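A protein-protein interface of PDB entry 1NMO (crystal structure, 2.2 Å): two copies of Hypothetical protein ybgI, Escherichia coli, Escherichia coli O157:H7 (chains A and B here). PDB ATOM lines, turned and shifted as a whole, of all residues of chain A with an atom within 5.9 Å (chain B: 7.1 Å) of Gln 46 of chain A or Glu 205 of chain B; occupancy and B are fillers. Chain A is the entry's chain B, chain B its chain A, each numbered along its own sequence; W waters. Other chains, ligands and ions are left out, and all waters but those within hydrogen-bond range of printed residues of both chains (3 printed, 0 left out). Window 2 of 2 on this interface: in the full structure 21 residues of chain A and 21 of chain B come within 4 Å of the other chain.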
ATOM      1  N   ALA A  44     -29.119 -21.924  29.628  1.00  0.00           N
ATOM      2  CA  ALA A  44     -30.469 -21.572  29.177  1.00  0.00           C
ATOM      3  C   ALA A  44     -30.487 -20.176  28.600  1.00  0.00           C
ATOM      4  O   ALA A  44     -31.278 -19.370  29.061  1.00  0.00           O
ATOM      5  CB  ALA A  44     -31.464 -21.620  30.379  1.00  0.00           C
ATOM      6  N   SER A  45     -29.698 -19.892  27.563  1.00  0.00           N
ATOM      7  CA  SER A  45     -29.665 -18.556  27.001  1.00  0.00           C
ATOM      8  C   SER A  45     -30.874 -18.294  26.113  1.00  0.00           C
ATOM      9  O   SER A  45     -31.621 -19.203  25.801  1.00  0.00           O
ATOM     10  CB  SER A  45     -28.403 -18.371  26.198  1.00  0.00           C
ATOM     11  OG  SER A  45     -28.561 -19.290  25.193  1.00  0.00           O
ATOM     12  N   GLN A  46     -31.063 -17.050  25.692  1.00  0.00           N
ATOM     13  CA  GLN A  46     -32.185 -16.726  24.827  1.00  0.00           C
ATOM     14  C   GLN A  46     -32.094 -17.555  23.519  1.00  0.00           C
ATOM     15  O   GLN A  46     -33.104 -17.992  22.949  1.00  0.00           O
ATOM     16  CB  GLN A  46     -32.162 -15.232  24.430  1.00  0.00           C
ATOM     17  CG  GLN A  46     -33.449 -14.793  23.658  1.00  0.00           C
ATOM     18  CD  GLN A  46     -34.707 -15.044  24.500  1.00  0.00           C
ATOM     19  OE1 GLN A  46     -34.872 -14.465  25.588  1.00  0.00           O
ATOM     20  NE2 GLN A  46     -35.620 -15.894  23.995  1.00  0.00           N
ATOM     21  N   ALA A  47     -30.876 -17.649  23.011  1.00  0.00           N
ATOM     22  CA  ALA A  47     -30.492 -18.345  21.787  1.00  0.00           C
ATOM     23  C   ALA A  47     -30.888 -19.804  21.904  1.00  0.00           C
ATOM     24  O   ALA A  47     -31.551 -20.312  21.007  1.00  0.00           O
ATOM     25  CB  ALA A  47     -28.958 -18.207  21.625  1.00  0.00           C
ATOM     26  N   LEU A  48     -30.507 -20.489  22.986  1.00  0.00           N
ATOM     27  CA  LEU A  48     -30.904 -21.884  23.182  1.00  0.00           C
ATOM     28  C   LEU A  48     -32.454 -21.966  23.220  1.00  0.00           C
ATOM     29  O   LEU A  48     -33.093 -22.789  22.503  1.00  0.00           O
ATOM     30  CB  LEU A  48     -30.332 -22.401  24.489  1.00  0.00           C
ATOM     31  CG  LEU A  48     -30.015 -23.907  24.770  1.00  0.00           C
ATOM     32  CD1 LEU A  48     -31.124 -24.520  25.487  1.00  0.00           C
ATOM     33  CD2 LEU A  48     -29.685 -24.686  23.506  1.00  0.00           C
ATOM     34  N   LEU A  49     -33.087 -21.124  24.037  1.00  0.00           N
ATOM     35  CA  LEU A  49     -34.541 -21.121  24.110  1.00  0.00           C
ATOM     36  C   LEU A  49     -35.246 -20.875  22.772  1.00  0.00           C
ATOM     37  O   LEU A  49     -36.314 -21.428  22.521  1.00  0.00           O
ATOM     38  CB  LEU A  49     -34.982 -20.061  25.081  1.00  0.00           C
ATOM     39  CG  LEU A  49     -35.226 -20.433  26.503  1.00  0.00           C
ATOM     40  CD1 LEU A  49     -34.595 -21.674  26.932  1.00  0.00           C
ATOM     41  CD2 LEU A  49     -34.834 -19.262  27.275  1.00  0.00           C
ATOM     42  N   ASP A  50     -34.693 -20.056  21.901  1.00  0.00           N
ATOM     43  CA  ASP A  50     -35.384 -19.843  20.625  1.00  0.00           C
ATOM     44  C   ASP A  50     -35.342 -21.101  19.751  1.00  0.00           C
ATOM     45  O   ASP A  50     -36.247 -21.362  18.938  1.00  0.00           O
ATOM     46  CB  ASP A  50     -34.762 -18.665  19.903  1.00  0.00           C
ATOM     47  CG  ASP A  50     -35.065 -17.349  20.594  1.00  0.00           C
ATOM     48  OD1 ASP A  50     -36.043 -17.321  21.415  1.00  0.00           O
ATOM     49  OD2 ASP A  50     -34.350 -16.337  20.327  1.00  0.00           O
ATOM     50  N   GLU A  51     -34.266 -21.878  19.897  1.00  0.00           N
ATOM     51  CA  GLU A  51     -34.105 -23.104  19.139  1.00  0.00           C
ATOM     52  C   GLU A  51     -35.080 -24.125  19.672  1.00  0.00           C
ATOM     53  O   GLU A  51     -35.679 -24.876  18.912  1.00  0.00           O
ATOM     54  CB  GLU A  51     -32.701 -23.603  19.345  1.00  0.00           C
ATOM     55  CG  GLU A  51     -31.804 -22.766  18.569  1.00  0.00           C
ATOM     56  CD  GLU A  51     -32.339 -22.777  17.199  1.00  0.00           C
ATOM     57  OE1 GLU A  51     -32.268 -23.920  16.626  1.00  0.00           O
ATOM     58  OE2 GLU A  51     -32.840 -21.676  16.752  1.00  0.00           O
ATOM     59  N   MET A  78     -33.682  -9.300  30.321  1.00  0.00           N
ATOM     60  CA  MET A  78     -33.392 -10.680  29.930  1.00  0.00           C
ATOM     61  C   MET A  78     -34.259 -11.723  30.554  1.00  0.00           C
ATOM     62  O   MET A  78     -34.711 -12.699  29.876  1.00  0.00           O
ATOM     63  CB  MET A  78     -31.927 -11.012  30.254  1.00  0.00           C
ATOM     64  CG  MET A  78     -30.973 -10.317  29.318  1.00  0.00           C
ATOM     65  SD  MET A  78     -29.223 -10.540  30.125  1.00  0.00           S
ATOM     66  CE  MET A  78     -28.708 -12.348  29.552  1.00  0.00           C
ATOM     67  N   ASN A  81     -37.693 -11.801  29.053  1.00  0.00           N
ATOM     68  CA  ASN A  81     -37.582 -12.385  27.698  1.00  0.00           C
ATOM     69  C   ASN A  81     -37.535 -13.906  27.642  1.00  0.00           C
ATOM     70  O   ASN A  81     -38.247 -14.573  26.822  1.00  0.00           O
ATOM     71  CB  ASN A  81     -36.319 -11.878  27.037  1.00  0.00           C
ATOM     72  CG  ASN A  81     -36.476 -10.481  26.538  1.00  0.00           C
ATOM     73  OD1 ASN A  81     -37.608  -9.948  26.504  1.00  0.00           O
ATOM     74  ND2 ASN A  81     -35.378  -9.871  26.116  1.00  0.00           N
ATOM     75  N   ARG A  82     -36.619 -14.427  28.453  1.00  0.00           N
ATOM     76  CA  ARG A  82     -36.389 -15.859  28.572  1.00  0.00           C
ATOM     77  C   ARG A  82     -37.596 -16.602  29.171  1.00  0.00           C
ATOM     78  O   ARG A  82     -38.052 -17.620  28.611  1.00  0.00           O
ATOM     79  CB  ARG A  82     -35.158 -16.107  29.463  1.00  0.00           C
ATOM     80  CG  ARG A  82     -33.828 -15.620  28.843  1.00  0.00           C
ATOM     81  CD  ARG A  82     -32.713 -15.619  29.928  1.00  0.00           C
ATOM     82  NE  ARG A  82     -31.427 -15.494  29.255  1.00  0.00           N
ATOM     83  CZ  ARG A  82     -30.262 -15.736  29.838  1.00  0.00           C
ATOM     84  NH1 ARG A  82     -30.216 -16.106  31.113  1.00  0.00           N
ATOM     85  NH2 ARG A  82     -29.153 -15.636  29.132  1.00  0.00           N
ATOM     86  N   THR A  85     -40.573 -16.669  26.749  1.00  0.00           N
ATOM     87  CA  THR A  85     -40.362 -17.655  25.680  1.00  0.00           C
ATOM     88  C   THR A  85     -40.644 -19.075  26.185  1.00  0.00           C
ATOM     89  O   THR A  85     -41.112 -19.926  25.416  1.00  0.00           O
ATOM     90  CB  THR A  85     -38.943 -17.668  25.105  1.00  0.00           C
ATOM     91  OG1 THR A  85     -38.630 -16.388  24.510  1.00  0.00           O
ATOM     92  CG2 THR A  85     -38.874 -18.779  24.024  1.00  0.00           C
ATOM     93  N   THR B 160     -24.206  -7.997  18.610  1.00  0.00           N
ATOM     94  CA  THR B 160     -25.490  -7.268  18.638  1.00  0.00           C
ATOM     95  C   THR B 160     -25.408  -5.853  19.168  1.00  0.00           C
ATOM     96  O   THR B 160     -26.425  -5.274  19.632  1.00  0.00           O
ATOM     97  CB  THR B 160     -26.547  -8.043  19.446  1.00  0.00           C
ATOM     98  OG1 THR B 160     -26.198  -8.020  20.840  1.00  0.00           O
ATOM     99  CG2 THR B 160     -26.585  -9.562  18.979  1.00  0.00           C
ATOM    100  N   THR B 199     -21.444 -13.398  31.255  1.00  0.00           N
ATOM    101  CA  THR B 199     -21.175 -12.073  30.690  1.00  0.00           C
ATOM    102  C   THR B 199     -21.509 -12.021  29.187  1.00  0.00           C
ATOM    103  O   THR B 199     -22.091 -11.039  28.676  1.00  0.00           O
ATOM    104  CB  THR B 199     -19.668 -11.710  30.801  1.00  0.00           C
ATOM    105  OG1 THR B 199     -19.123 -12.100  32.083  1.00  0.00           O
ATOM    106  CG2 THR B 199     -19.497 -10.197  30.607  1.00  0.00           C
ATOM    107  N   ILE B 200     -21.078 -13.045  28.446  1.00  0.00           N
ATOM    108  CA  ILE B 200     -21.356 -13.128  27.001  1.00  0.00           C
ATOM    109  C   ILE B 200     -22.870 -13.109  26.618  1.00  0.00           C
ATOM    110  O   ILE B 200     -23.280 -12.524  25.603  1.00  0.00           O
ATOM    111  CB  ILE B 200     -20.700 -14.441  26.414  1.00  0.00           C
ATOM    112  CG1 ILE B 200     -19.190 -14.373  26.594  1.00  0.00           C
ATOM    113  CG2 ILE B 200     -20.993 -14.548  24.940  1.00  0.00           C
ATOM    114  CD1 ILE B 200     -18.611 -13.164  25.931  1.00  0.00           C
ATOM    115  N   HIS B 201     -23.703 -13.767  27.402  1.00  0.00           N
ATOM    116  CA  HIS B 201     -25.148 -13.752  27.075  1.00  0.00           C
ATOM    117  C   HIS B 201     -25.693 -12.353  27.397  1.00  0.00           C
ATOM    118  O   HIS B 201     -26.689 -11.855  26.793  1.00  0.00           O
ATOM    119  CB  HIS B 201     -25.899 -14.817  27.925  1.00  0.00           C
ATOM    120  CG  HIS B 201     -25.281 -16.180  27.853  1.00  0.00           C
ATOM    121  ND1 HIS B 201     -25.018 -16.804  26.650  1.00  0.00           N
ATOM    122  CD2 HIS B 201     -24.774 -16.993  28.815  1.00  0.00           C
ATOM    123  CE1 HIS B 201     -24.374 -17.946  26.873  1.00  0.00           C
ATOM    124  NE2 HIS B 201     -24.213 -18.080  28.178  1.00  0.00           N
ATOM    125  N   SER B 202     -25.098 -11.717  28.397  1.00  0.00           N
ATOM    126  CA  SER B 202     -25.571 -10.361  28.705  1.00  0.00           C
ATOM    127  C   SER B 202     -25.250  -9.415  27.566  1.00  0.00           C
ATOM    128  O   SER B 202     -26.096  -8.629  27.184  1.00  0.00           O
ATOM    129  CB  SER B 202     -24.935  -9.830  29.987  1.00  0.00           C
ATOM    130  OG  SER B 202     -25.320 -10.633  31.098  1.00  0.00           O
ATOM    131  N   ALA B 203     -24.043  -9.506  27.004  1.00  0.00           N
ATOM    132  CA  ALA B 203     -23.619  -8.634  25.911  1.00  0.00           C
ATOM    133  C   ALA B 203     -24.533  -8.812  24.744  1.00  0.00           C
ATOM    134  O   ALA B 203     -25.069  -7.817  24.165  1.00  0.00           O
ATOM    135  CB  ALA B 203     -22.210  -8.983  25.482  1.00  0.00           C
ATOM    136  N   ARG B 204     -24.730 -10.094  24.407  1.00  0.00           N
ATOM    137  CA  ARG B 204     -25.568 -10.471  23.290  1.00  0.00           C
ATOM    138  C   ARG B 204     -27.068 -10.107  23.435  1.00  0.00           C
ATOM    139  O   ARG B 204     -27.642  -9.511  22.534  1.00  0.00           O
ATOM    140  CB  ARG B 204     -25.459 -11.995  23.036  1.00  0.00           C
ATOM    141  CG  ARG B 204     -24.173 -12.441  22.350  1.00  0.00           C
ATOM    142  CD  ARG B 204     -24.064 -14.033  22.349  1.00  0.00           C
ATOM    143  NE  ARG B 204     -22.788 -14.492  21.749  1.00  0.00           N
ATOM    144  CZ  ARG B 204     -22.407 -15.777  21.754  1.00  0.00           C
ATOM    145  NH1 ARG B 204     -23.203 -16.695  22.326  1.00  0.00           N
ATOM    146  NH2 ARG B 204     -21.257 -16.179  21.157  1.00  0.00           N
ATOM    147  N   GLU B 205     -27.672 -10.487  24.560  1.00  0.00           N
ATOM    148  CA  GLU B 205     -29.095 -10.295  24.779  1.00  0.00           C
ATOM    149  C   GLU B 205     -29.566  -8.890  25.076  1.00  0.00           C
ATOM    150  O   GLU B 205     -30.764  -8.580  24.959  1.00  0.00           O
ATOM    151  CB  GLU B 205     -29.560 -11.281  25.845  1.00  0.00           C
ATOM    152  CG  GLU B 205     -29.643 -12.726  25.245  1.00  0.00           C
ATOM    153  CD  GLU B 205     -29.969 -13.803  26.330  1.00  0.00           C
ATOM    154  OE1 GLU B 205     -30.854 -13.595  27.200  1.00  0.00           O
ATOM    155  OE2 GLU B 205     -29.323 -14.873  26.347  1.00  0.00           O
ATOM    156  N   GLN B 206     -28.626  -8.025  25.435  1.00  0.00           N
ATOM    157  CA  GLN B 206     -28.969  -6.632  25.704  1.00  0.00           C
ATOM    158  C   GLN B 206     -28.375  -5.705  24.646  1.00  0.00           C
ATOM    159  O   GLN B 206     -28.478  -4.493  24.782  1.00  0.00           O
ATOM    160  CB  GLN B 206     -28.577  -6.224  27.146  1.00  0.00           C
ATOM    161  CG  GLN B 206     -29.489  -6.905  28.218  1.00  0.00           C
ATOM    162  CD  GLN B 206     -28.909  -6.897  29.688  1.00  0.00           C
ATOM    163  OE1 GLN B 206     -27.675  -6.923  29.905  1.00  0.00           O
ATOM    164  NE2 GLN B 206     -29.803  -6.926  30.688  1.00  0.00           N
ATOM    165  N   GLY B 207     -27.775  -6.256  23.583  1.00  0.00           N
ATOM    166  CA  GLY B 207     -27.254  -5.390  22.519  1.00  0.00           C
ATOM    167  C   GLY B 207     -26.109  -4.386  22.773  1.00  0.00           C
ATOM    168  O   GLY B 207     -26.090  -3.261  22.249  1.00  0.00           O
ATOM    169  N   LEU B 208     -25.111  -4.747  23.581  1.00  0.00           N
ATOM    170  CA  LEU B 208     -24.012  -3.810  23.739  1.00  0.00           C
ATOM    171  C   LEU B 208     -22.690  -4.524  23.422  1.00  0.00           C
ATOM    172  O   LEU B 208     -22.614  -5.748  23.418  1.00  0.00           O
ATOM    173  CB  LEU B 208     -23.980  -3.194  25.124  1.00  0.00           C
ATOM    174  CG  LEU B 208     -23.789  -4.164  26.270  1.00  0.00           C
ATOM    175  CD1 LEU B 208     -23.514  -3.419  27.593  1.00  0.00           C
ATOM    176  CD2 LEU B 208     -25.035  -4.924  26.413  1.00  0.00           C
HETATM  177  O   HOH W   1     -28.492 -15.618  23.594  1.00  0.00           O
HETATM  178  O   HOH W   2     -33.185 -12.385  26.109  1.00  0.00           O
HETATM  179  O   HOH W   3     -27.739 -11.638  33.247  1.00  0.00           O
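NE of Arg 82 of chain A lies within salt-bridge range of OE1 of Glu 205 of chain B (2.9 Å). The backbone NH of Gln 46 of chain A is in hydrogen-bond range of the side-chain carboxylate of Glu 205 of chain B (2.9 Å). The side-chain sulfur (SD) of Met 78 of chain A sits close to the side-chain amide nitrogen (NE2) of Gln 206 of chain B (3.7 Å).
Gln 46 of chain A touches just one residue of chain B: Glu 205. Glu 205 of chain B touches just these residues of chain A: Ser 45 (3.6 Å), Gln 46 (2.9 Å), Met 78 (3.4 Å) and Arg 82 (2.9 Å). Of the printed residues of chain A, Gln 206 of chain B touches Met 78. Printed residues of chain A within 4 Å of Ser 202 of chain B: Met 78. Leu 48 of chain A touches none of the printed residues of chain B. The nearest residue of chain B that does not touch Gln 46 of chain A is His 201 of chain B (6.1 Å).
The side-chain carboxylate (OD1) of Asp 50 of chain A lies within hydrogen-bond range of the side-chain amide nitrogen (NE2) of Gln 46 of chain A. The backbone NH (N) of Arg 82 of chain A is in hydrogen-bond range of the side-chain amide oxygen (OE1) of Gln 46 of chain A (3.4 Å). OG of Ser 45 of chain A sits at hydrogen-bond distance from N of Leu 48 of chain A, at 3.2 Å. NE2 of Gln 46 of chain A lies within hydrogen-bond range of OG1 of Thr 85 of chain A (3.1 Å).
No position is printed for both chains.
Of the 12 printed residues of chain A, 4 touch a printed residue of chain B. Hydrophobic or aromatic side chains of chain A within 4 Å of the printed part of chain B: Met 78. Printed residues of chain B that touch a printed residue of chain A: His 201, Ser 202, Glu 205 and Gln 206. Hydrophobic or aromatic side chains of chain B within 4 Å of the printed part of chain A: His 201. Among the printed residues, 9 pairs touch across the chains.
Water W2 lies within hydrogen-bond range of the side-chain amide oxygen of Gln 46 of chain A (2.7 Å), the side-chain carboxylate of Glu 205 of chain B (2.8 Å) and the side-chain amide nitrogen of Asn 81 of chain A (3.3 Å). Water W1 bridges OE2 of Glu 205 of chain B (3.0 Å) and N of Ala 47 of chain A (3.2 Å). Water W3 bridges the side-chain hydroxyl of Ser 202 of chain B and the side-chain sulfur of Met 78 of chain A.
Among the printed residues, pairs that only touch across the chains: Met 78 of chain A with Glu 205 of chain B, Met 78 of chain A with His 201 of chain B, Arg 82 of chain A with His 201 of chain B, Ser 45 of chain A with Glu 205 of chain B, Ser 45 of chain A with His 201 of chain B and Met 78 of chain A with Ser 202 of chain B.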
